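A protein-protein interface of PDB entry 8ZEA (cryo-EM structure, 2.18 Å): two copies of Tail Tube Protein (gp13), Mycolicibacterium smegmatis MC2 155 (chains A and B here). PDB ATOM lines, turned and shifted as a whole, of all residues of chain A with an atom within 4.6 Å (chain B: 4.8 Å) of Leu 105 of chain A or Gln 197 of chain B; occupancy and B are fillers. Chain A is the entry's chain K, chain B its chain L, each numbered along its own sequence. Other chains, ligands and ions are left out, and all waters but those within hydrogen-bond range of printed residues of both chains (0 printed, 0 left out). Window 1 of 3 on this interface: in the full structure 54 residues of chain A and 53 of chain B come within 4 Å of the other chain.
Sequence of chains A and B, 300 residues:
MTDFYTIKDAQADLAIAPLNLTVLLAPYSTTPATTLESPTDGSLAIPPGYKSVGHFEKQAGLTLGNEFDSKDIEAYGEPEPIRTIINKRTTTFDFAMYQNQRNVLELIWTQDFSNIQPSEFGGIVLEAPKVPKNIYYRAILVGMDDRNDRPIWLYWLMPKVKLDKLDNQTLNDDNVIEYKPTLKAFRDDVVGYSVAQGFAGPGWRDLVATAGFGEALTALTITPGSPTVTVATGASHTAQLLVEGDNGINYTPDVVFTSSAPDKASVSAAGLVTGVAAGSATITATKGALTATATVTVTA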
ATOM      1  N   ASN A 100     -17.124 -22.801  10.614  1.00  0.00           N
ATOM      2  CA  ASN A 100     -17.066 -21.934   9.439  1.00  0.00           C
ATOM      3  C   ASN A 100     -15.920 -20.935   9.591  1.00  0.00           C
ATOM      4  O   ASN A 100     -16.109 -19.727   9.733  1.00  0.00           O
ATOM      5  CB  ASN A 100     -18.400 -21.229   9.236  1.00  0.00           C
ATOM      6  CG  ASN A 100     -19.485 -22.168   8.776  1.00  0.00           C
ATOM      7  OD1 ASN A 100     -19.639 -22.411   7.585  1.00  0.00           O
ATOM      8  ND2 ASN A 100     -20.239 -22.711   9.721  1.00  0.00           N
ATOM      9  N   GLN A 101     -14.708 -21.469   9.564  1.00  0.00           N
ATOM     10  CA  GLN A 101     -13.505 -20.659   9.646  1.00  0.00           C
ATOM     11  C   GLN A 101     -12.775 -20.682   8.310  1.00  0.00           C
ATOM     12  O   GLN A 101     -13.124 -21.428   7.393  1.00  0.00           O
ATOM     13  CB  GLN A 101     -12.591 -21.137  10.776  1.00  0.00           C
ATOM     14  CG  GLN A 101     -12.371 -22.627  10.829  1.00  0.00           C
ATOM     15  CD  GLN A 101     -11.694 -23.054  12.111  1.00  0.00           C
ATOM     16  OE1 GLN A 101     -12.098 -22.650  13.198  1.00  0.00           O
ATOM     17  NE2 GLN A 101     -10.657 -23.866  11.993  1.00  0.00           N
ATOM     18  N   ARG A 102     -11.741 -19.846   8.217  1.00  0.00           N
ATOM     19  CA  ARG A 102     -11.122 -19.582   6.924  1.00  0.00           C
ATOM     20  C   ARG A 102     -10.454 -20.823   6.340  1.00  0.00           C
ATOM     21  O   ARG A 102     -10.570 -21.077   5.141  1.00  0.00           O
ATOM     22  CB  ARG A 102     -10.117 -18.439   7.039  1.00  0.00           C
ATOM     23  CG  ARG A 102      -9.405 -18.141   5.733  1.00  0.00           C
ATOM     24  CD  ARG A 102      -8.927 -16.709   5.665  1.00  0.00           C
ATOM     25  NE  ARG A 102      -7.824 -16.468   6.585  1.00  0.00           N
ATOM     26  CZ  ARG A 102      -6.586 -16.908   6.406  1.00  0.00           C
ATOM     27  NH1 ARG A 102      -6.247 -17.605   5.335  1.00  0.00           N
ATOM     28  NH2 ARG A 102      -5.666 -16.641   7.327  1.00  0.00           N
ATOM     29  N   ASN A 103      -9.744 -21.603   7.158  1.00  0.00           N
ATOM     30  CA  ASN A 103      -9.004 -22.731   6.594  1.00  0.00           C
ATOM     31  C   ASN A 103      -9.946 -23.817   6.076  1.00  0.00           C
ATOM     32  O   ASN A 103      -9.695 -24.406   5.017  1.00  0.00           O
ATOM     33  CB  ASN A 103      -8.000 -23.284   7.613  1.00  0.00           C
ATOM     34  CG  ASN A 103      -8.645 -23.750   8.906  1.00  0.00           C
ATOM     35  OD1 ASN A 103      -9.796 -23.438   9.192  1.00  0.00           O
ATOM     36  ND2 ASN A 103      -7.890 -24.495   9.700  1.00  0.00           N
ATOM     37  N   VAL A 104     -11.060 -24.056   6.771  1.00  0.00           N
ATOM     38  CA  VAL A 104     -12.048 -25.029   6.305  1.00  0.00           C
ATOM     39  C   VAL A 104     -12.649 -24.594   4.969  1.00  0.00           C
ATOM     40  O   VAL A 104     -12.764 -25.389   4.028  1.00  0.00           O
ATOM     41  CB  VAL A 104     -13.140 -25.233   7.372  1.00  0.00           C
ATOM     42  CG1 VAL A 104     -14.276 -26.087   6.830  1.00  0.00           C
ATOM     43  CG2 VAL A 104     -12.549 -25.842   8.634  1.00  0.00           C
ATOM     44  N   LEU A 105     -13.049 -23.324   4.873  1.00  0.00           N
ATOM     45  CA  LEU A 105     -13.681 -22.835   3.651  1.00  0.00           C
ATOM     46  C   LEU A 105     -12.685 -22.765   2.499  1.00  0.00           C
ATOM     47  O   LEU A 105     -13.038 -23.045   1.348  1.00  0.00           O
ATOM     48  CB  LEU A 105     -14.326 -21.474   3.906  1.00  0.00           C
ATOM     49  CG  LEU A 105     -15.505 -21.529   4.880  1.00  0.00           C
ATOM     50  CD1 LEU A 105     -15.709 -20.203   5.590  1.00  0.00           C
ATOM     51  CD2 LEU A 105     -16.771 -21.965   4.156  1.00  0.00           C
ATOM     52  N   GLU A 106     -11.437 -22.406   2.794  1.00  0.00           N
ATOM     53  CA  GLU A 106     -10.383 -22.438   1.789  1.00  0.00           C
ATOM     54  C   GLU A 106     -10.183 -23.847   1.256  1.00  0.00           C
ATOM     55  O   GLU A 106     -10.016 -24.044   0.048  1.00  0.00           O
ATOM     56  CB  GLU A 106      -9.081 -21.902   2.383  1.00  0.00           C
ATOM     57  CG  GLU A 106      -8.946 -20.398   2.340  1.00  0.00           C
ATOM     58  CD  GLU A 106      -7.731 -19.900   3.091  1.00  0.00           C
ATOM     59  OE1 GLU A 106      -7.133 -20.693   3.847  1.00  0.00           O
ATOM     60  OE2 GLU A 106      -7.364 -18.719   2.917  1.00  0.00           O
ATOM     61  N   LEU A 107     -10.201 -24.842   2.145  1.00  0.00           N
ATOM     62  CA  LEU A 107     -10.085 -26.225   1.705  1.00  0.00           C
ATOM     63  C   LEU A 107     -11.252 -26.618   0.806  1.00  0.00           C
ATOM     64  O   LEU A 107     -11.050 -27.163  -0.285  1.00  0.00           O
ATOM     65  CB  LEU A 107      -9.999 -27.152   2.917  1.00  0.00           C
ATOM     66  CG  LEU A 107     -10.100 -28.648   2.623  1.00  0.00           C
ATOM     67  CD1 LEU A 107      -8.893 -29.111   1.826  1.00  0.00           C
ATOM     68  CD2 LEU A 107     -10.249 -29.450   3.903  1.00  0.00           C
ATOM     69  N   ILE A 108     -12.483 -26.337   1.239  1.00  0.00           N
ATOM     70  CA  ILE A 108     -13.634 -26.838   0.490  1.00  0.00           C
ATOM     71  C   ILE A 108     -13.790 -26.118  -0.846  1.00  0.00           C
ATOM     72  O   ILE A 108     -14.268 -26.711  -1.817  1.00  0.00           O
ATOM     73  CB  ILE A 108     -14.933 -26.745   1.311  1.00  0.00           C
ATOM     74  CG1 ILE A 108     -15.279 -25.285   1.585  1.00  0.00           C
ATOM     75  CG2 ILE A 108     -14.822 -27.569   2.588  1.00  0.00           C
ATOM     76  CD1 ILE A 108     -16.676 -25.066   2.014  1.00  0.00           C
ATOM     77  N   TRP A 109     -13.410 -24.845  -0.926  1.00  0.00           N
ATOM     78  CA  TRP A 109     -13.572 -24.092  -2.163  1.00  0.00           C
ATOM     79  C   TRP A 109     -12.318 -24.071  -3.029  1.00  0.00           C
ATOM     80  O   TRP A 109     -12.328 -23.413  -4.072  1.00  0.00           O
ATOM     81  CB  TRP A 109     -14.017 -22.660  -1.855  1.00  0.00           C
ATOM     82  CG  TRP A 109     -15.437 -22.579  -1.393  1.00  0.00           C
ATOM     83  CD1 TRP A 109     -15.881 -22.143  -0.183  1.00  0.00           C
ATOM     84  CD2 TRP A 109     -16.604 -22.964  -2.132  1.00  0.00           C
ATOM     85  NE1 TRP A 109     -17.246 -22.224  -0.121  1.00  0.00           N
ATOM     86  CE2 TRP A 109     -17.717 -22.726  -1.305  1.00  0.00           C
ATOM     87  CE3 TRP A 109     -16.815 -23.481  -3.414  1.00  0.00           C
ATOM     88  CZ2 TRP A 109     -19.023 -22.988  -1.715  1.00  0.00           C
ATOM     89  CZ3 TRP A 109     -18.111 -23.744  -3.819  1.00  0.00           C
ATOM     90  CH2 TRP A 109     -19.198 -23.497  -2.973  1.00  0.00           C
ATOM     91  N   PHE A 113      -8.141 -17.540   0.608  1.00  0.00           N
ATOM     92  CA  PHE A 113      -9.009 -16.450   1.036  1.00  0.00           C
ATOM     93  C   PHE A 113      -8.308 -15.488   1.987  1.00  0.00           C
ATOM     94  O   PHE A 113      -8.972 -14.693   2.656  1.00  0.00           O
ATOM     95  CB  PHE A 113     -10.276 -17.003   1.689  1.00  0.00           C
ATOM     96  CG  PHE A 113     -11.235 -17.633   0.724  1.00  0.00           C
ATOM     97  CD1 PHE A 113     -11.558 -17.002  -0.464  1.00  0.00           C
ATOM     98  CD2 PHE A 113     -11.818 -18.858   1.006  1.00  0.00           C
ATOM     99  CE1 PHE A 113     -12.443 -17.578  -1.350  1.00  0.00           C
ATOM    100  CE2 PHE A 113     -12.700 -19.438   0.125  1.00  0.00           C
ATOM    101  CZ  PHE A 113     -13.013 -18.798  -1.058  1.00  0.00           C
ATOM    102  N   ILE A 124     -18.625 -11.128   4.762  1.00  0.00           N
ATOM    103  CA  ILE A 124     -17.664 -11.624   3.787  1.00  0.00           C
ATOM    104  C   ILE A 124     -18.410 -12.365   2.691  1.00  0.00           C
ATOM    105  O   ILE A 124     -19.476 -12.943   2.917  1.00  0.00           O
ATOM    106  CB  ILE A 124     -16.593 -12.542   4.425  1.00  0.00           C
ATOM    107  CG1 ILE A 124     -17.249 -13.736   5.119  1.00  0.00           C
ATOM    108  CG2 ILE A 124     -15.707 -11.761   5.385  1.00  0.00           C
ATOM    109  CD1 ILE A 124     -16.338 -14.926   5.268  1.00  0.00           C
ATOM    110  N   VAL A 125     -17.841 -12.336   1.492  1.00  0.00           N
ATOM    111  CA  VAL A 125     -18.334 -13.105   0.358  1.00  0.00           C
ATOM    112  C   VAL A 125     -17.161 -13.882  -0.220  1.00  0.00           C
ATOM    113  O   VAL A 125     -16.138 -13.291  -0.579  1.00  0.00           O
ATOM    114  CB  VAL A 125     -18.978 -12.206  -0.716  1.00  0.00           C
ATOM    115  CG1 VAL A 125     -19.392 -13.033  -1.923  1.00  0.00           C
ATOM    116  CG2 VAL A 125     -20.177 -11.472  -0.146  1.00  0.00           C
ATOM    117  N   LEU A 126     -17.305 -15.199  -0.300  1.00  0.00           N
ATOM    118  CA  LEU A 126     -16.259 -16.084  -0.803  1.00  0.00           C
ATOM    119  C   LEU A 126     -16.727 -16.674  -2.126  1.00  0.00           C
ATOM    120  O   LEU A 126     -17.627 -17.517  -2.151  1.00  0.00           O
ATOM    121  CB  LEU A 126     -15.939 -17.182   0.209  1.00  0.00           C
ATOM    122  CG  LEU A 126     -15.631 -16.717   1.634  1.00  0.00           C
ATOM    123  CD1 LEU A 126     -15.620 -17.889   2.598  1.00  0.00           C
ATOM    124  CD2 LEU A 126     -14.314 -15.961   1.684  1.00  0.00           C
ATOM    125  N   TYR A 179     -19.263 -29.703   6.498  1.00  0.00           N
ATOM    126  CA  TYR A 179     -18.424 -29.840   5.317  1.00  0.00           C
ATOM    127  C   TYR A 179     -17.710 -31.181   5.411  1.00  0.00           C
ATOM    128  O   TYR A 179     -17.029 -31.455   6.404  1.00  0.00           O
ATOM    129  CB  TYR A 179     -17.427 -28.686   5.215  1.00  0.00           C
ATOM    130  CG  TYR A 179     -18.070 -27.322   5.288  1.00  0.00           C
ATOM    131  CD1 TYR A 179     -18.669 -26.758   4.172  1.00  0.00           C
ATOM    132  CD2 TYR A 179     -18.088 -26.603   6.471  1.00  0.00           C
ATOM    133  CE1 TYR A 179     -19.258 -25.510   4.232  1.00  0.00           C
ATOM    134  CE2 TYR A 179     -18.673 -25.360   6.541  1.00  0.00           C
ATOM    135  CZ  TYR A 179     -19.257 -24.816   5.419  1.00  0.00           C
ATOM    136  OH  TYR A 179     -19.844 -23.578   5.485  1.00  0.00           O
ATOM    137  N   TYR B 155     -25.363 -17.460   3.316  1.00  0.00           N
ATOM    138  CA  TYR B 155     -26.045 -17.492   2.038  1.00  0.00           C
ATOM    139  C   TYR B 155     -25.124 -17.978   0.932  1.00  0.00           C
ATOM    140  O   TYR B 155     -23.899 -17.987   1.059  1.00  0.00           O
ATOM    141  CB  TYR B 155     -26.638 -16.125   1.669  1.00  0.00           C
ATOM    142  CG  TYR B 155     -25.673 -14.966   1.644  1.00  0.00           C
ATOM    143  CD1 TYR B 155     -25.347 -14.283   2.807  1.00  0.00           C
ATOM    144  CD2 TYR B 155     -25.127 -14.524   0.448  1.00  0.00           C
ATOM    145  CE1 TYR B 155     -24.489 -13.210   2.784  1.00  0.00           C
ATOM    146  CE2 TYR B 155     -24.270 -13.450   0.414  1.00  0.00           C
ATOM    147  CZ  TYR B 155     -23.953 -12.796   1.585  1.00  0.00           C
ATOM    148  OH  TYR B 155     -23.097 -11.726   1.552  1.00  0.00           O
ATOM    149  N   TRP B 156     -25.754 -18.404  -0.157  1.00  0.00           N
ATOM    150  CA  TRP B 156     -25.075 -18.802  -1.377  1.00  0.00           C
ATOM    151  C   TRP B 156     -25.648 -17.994  -2.528  1.00  0.00           C
ATOM    152  O   TRP B 156     -26.870 -17.894  -2.672  1.00  0.00           O
ATOM    153  CB  TRP B 156     -25.230 -20.301  -1.642  1.00  0.00           C
ATOM    154  CG  TRP B 156     -24.495 -21.163  -0.671  1.00  0.00           C
ATOM    155  CD1 TRP B 156     -23.286 -21.761  -0.861  1.00  0.00           C
ATOM    156  CD2 TRP B 156     -24.919 -21.527   0.646  1.00  0.00           C
ATOM    157  NE1 TRP B 156     -22.931 -22.474   0.253  1.00  0.00           N
ATOM    158  CE2 TRP B 156     -23.915 -22.345   1.194  1.00  0.00           C
ATOM    159  CE3 TRP B 156     -26.048 -21.237   1.415  1.00  0.00           C
ATOM    160  CZ2 TRP B 156     -24.009 -22.882   2.475  1.00  0.00           C
ATOM    161  CZ3 TRP B 156     -26.138 -21.765   2.685  1.00  0.00           C
ATOM    162  CH2 TRP B 156     -25.124 -22.580   3.203  1.00  0.00           C
ATOM    163  N   VAL B 195     -20.740 -19.877  -8.061  1.00  0.00           N
ATOM    164  CA  VAL B 195     -21.265 -19.956  -6.703  1.00  0.00           C
ATOM    165  C   VAL B 195     -20.401 -19.093  -5.797  1.00  0.00           C
ATOM    166  O   VAL B 195     -19.172 -19.092  -5.909  1.00  0.00           O
ATOM    167  CB  VAL B 195     -21.311 -21.411  -6.182  1.00  0.00           C
ATOM    168  CG1 VAL B 195     -21.915 -21.461  -4.791  1.00  0.00           C
ATOM    169  CG2 VAL B 195     -22.093 -22.299  -7.124  1.00  0.00           C
ATOM    170  N   ALA B 196     -21.047 -18.352  -4.904  1.00  0.00           N
ATOM    171  CA  ALA B 196     -20.365 -17.608  -3.856  1.00  0.00           C
ATOM    172  C   ALA B 196     -21.062 -17.861  -2.529  1.00  0.00           C
ATOM    173  O   ALA B 196     -22.292 -17.875  -2.460  1.00  0.00           O
ATOM    174  CB  ALA B 196     -20.333 -16.107  -4.161  1.00  0.00           C
ATOM    175  N   GLN B 197     -20.275 -18.062  -1.479  1.00  0.00           N
ATOM    176  CA  GLN B 197     -20.790 -18.273  -0.134  1.00  0.00           C
ATOM    177  C   GLN B 197     -20.571 -17.010   0.688  1.00  0.00           C
ATOM    178  O   GLN B 197     -19.481 -16.433   0.663  1.00  0.00           O
ATOM    179  CB  GLN B 197     -20.115 -19.476   0.529  1.00  0.00           C
ATOM    180  CG  GLN B 197     -20.742 -19.893   1.845  1.00  0.00           C
ATOM    181  CD  GLN B 197     -20.284 -21.260   2.318  1.00  0.00           C
ATOM    182  OE1 GLN B 197     -19.498 -21.929   1.653  1.00  0.00           O
ATOM    183  NE2 GLN B 197     -20.779 -21.681   3.470  1.00  0.00           N
ATOM    184  N   GLY B 198     -21.602 -16.583   1.404  1.00  0.00           N
ATOM    185  CA  GLY B 198     -21.540 -15.352   2.164  1.00  0.00           C
ATOM    186  C   GLY B 198     -21.958 -15.539   3.607  1.00  0.00           C
ATOM    187  O   GLY B 198     -22.763 -16.406   3.938  1.00  0.00           O
ATOM    188  N   PHE B 199     -21.384 -14.705   4.468  1.00  0.00           N
ATOM    189  CA  PHE B 199     -21.731 -14.638   5.882  1.00  0.00           C
ATOM    190  C   PHE B 199     -21.958 -13.181   6.248  1.00  0.00           C
ATOM    191  O   PHE B 199     -21.144 -12.324   5.898  1.00  0.00           O
ATOM    192  CB  PHE B 199     -20.630 -15.234   6.770  1.00  0.00           C
ATOM    193  CG  PHE B 199     -20.298 -16.662   6.458  1.00  0.00           C
ATOM    194  CD1 PHE B 199     -19.381 -16.975   5.471  1.00  0.00           C
ATOM    195  CD2 PHE B 199     -20.902 -17.694   7.153  1.00  0.00           C
ATOM    196  CE1 PHE B 199     -19.076 -18.285   5.182  1.00  0.00           C
ATOM    197  CE2 PHE B 199     -20.597 -19.010   6.869  1.00  0.00           C
ATOM    198  CZ  PHE B 199     -19.684 -19.306   5.884  1.00  0.00           C
ATOM    199  N   PHE B 213     -10.911 -14.328   9.309  1.00  0.00           N
ATOM    200  CA  PHE B 213     -10.998 -13.355   8.229  1.00  0.00           C
ATOM    201  C   PHE B 213     -10.676 -11.974   8.779  1.00  0.00           C
ATOM    202  O   PHE B 213     -11.303 -11.523   9.742  1.00  0.00           O
ATOM    203  CB  PHE B 213     -12.387 -13.366   7.589  1.00  0.00           C
ATOM    204  CG  PHE B 213     -12.780 -14.694   7.018  1.00  0.00           C
ATOM    205  CD1 PHE B 213     -12.346 -15.078   5.760  1.00  0.00           C
ATOM    206  CD2 PHE B 213     -13.586 -15.559   7.736  1.00  0.00           C
ATOM    207  CE1 PHE B 213     -12.710 -16.296   5.232  1.00  0.00           C
ATOM    208  CE2 PHE B 213     -13.953 -16.780   7.211  1.00  0.00           C
ATOM    209  CZ  PHE B 213     -13.516 -17.148   5.957  1.00  0.00           C
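OE1 of Gln 197 of chain B is in hydrogen-bond range of NE1 of Trp 109 of chain A, at 2.9 Å.
The backbone NH of Ile 124 of chain A lies within hydrogen-bond range of the backbone carbonyl oxygen of Phe 199 of chain B (3.0 Å).
N of Leu 126 of chain A lies within hydrogen-bond range of O of Gln 197 of chain B (2.7 Å).
OH of Tyr 179 of chain A sits at hydrogen-bond distance from NE2 of Gln 197 of chain B, at 2.9 Å.
The side-chain amide oxygen of Asn 100 of chain A is in hydrogen-bond range of the side-chain hydroxyl of Tyr 179 of chain A (2.4 Å).
The guanidinium group (NH1) of Arg 102 of chain A is in salt-bridge range of the side-chain carboxylate (OE2) of Glu 106 of chain A (2.9 Å).
The backbone carbonyl oxygen (O) of Tyr 155 of chain B sits at hydrogen-bond distance from the backbone NH (N) of Gly 198 of chain B.
CZ of Phe 199 of chain B touches OD1 of Asn 100 of chain A (3.5 Å).
CA of Arg 102 of chain A touches CZ of Phe 213 of chain B (3.5 Å).
CD2 of Leu 105 of chain A touches OE1 of Gln 197 of chain B, at 3.7 Å.
Phe 199 of chain B touches Leu 105 of chain A (CE1 to CD1, 3.9 Å).
CH2 of Trp 109 of chain A touches CG1 of Val 195 of chain B, at 3.9 Å.
CG2 of Val 125 of chain A touches OH of Tyr 155 of chain B, 3.4 Å away.
Ala 196 of chain B touches Val 125 of chain A.
Gln 197 of chain B touches Val 125 of chain A (O to CA, 3.5 Å).
Ala 196 of chain B touches Leu 126 of chain A.
Phe 213 of chain B touches Leu 126 of chain A.
Leu 105 of chain A touches just these residues of chain B: Gln 197 (3.7 Å), Phe 199 (3.9 Å) and Phe 213 (3.8 Å).
Leu 107 of chain A touches none of the printed residues of chain B.
Of the printed residues of chain B, Ile 124 of chain A touches Gly 198, Phe 199 and Phe 213.
Of the printed residues of chain B, Leu 126 of chain A touches Ala 196 (3.2 Å), Gln 197 (2.7 Å) and Phe 213 (3.9 Å).
Of the printed residues of chain A, Tyr 155 of chain B touches Val 125.
Of chain A, only Leu 105, Trp 109, Val 125, Leu 126 and Tyr 179 come within 4 Å of Gln 197 of chain B.
Of the printed residues of chain A, Phe 199 of chain B touches Asn 100, Leu 105 and Ile 124.
The nearest residue of chain A that does not touch Gln 197 of chain B is Ile 124 of chain A (4.2 Å).
The nearest printed residue of chain A that does not touch Phe 199 of chain B is Tyr 179 of chain A (4.3 Å).
Of the 15 printed residues of chain A, 8 touch a printed residue of chain B.
Hydrophobic or aromatic side chains of chain A that line the printed part of chain B: Leu 105, Trp 109, Ile 124, Val 125, Leu 126 and Tyr 179.
Of the 8 printed residues of chain B, 7 touch a printed residue of chain A.
No position is printed for both chains.
Of the 17 pairs that touch across the chains among the printed residues, none has its exchanged pair printed and touching as well.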
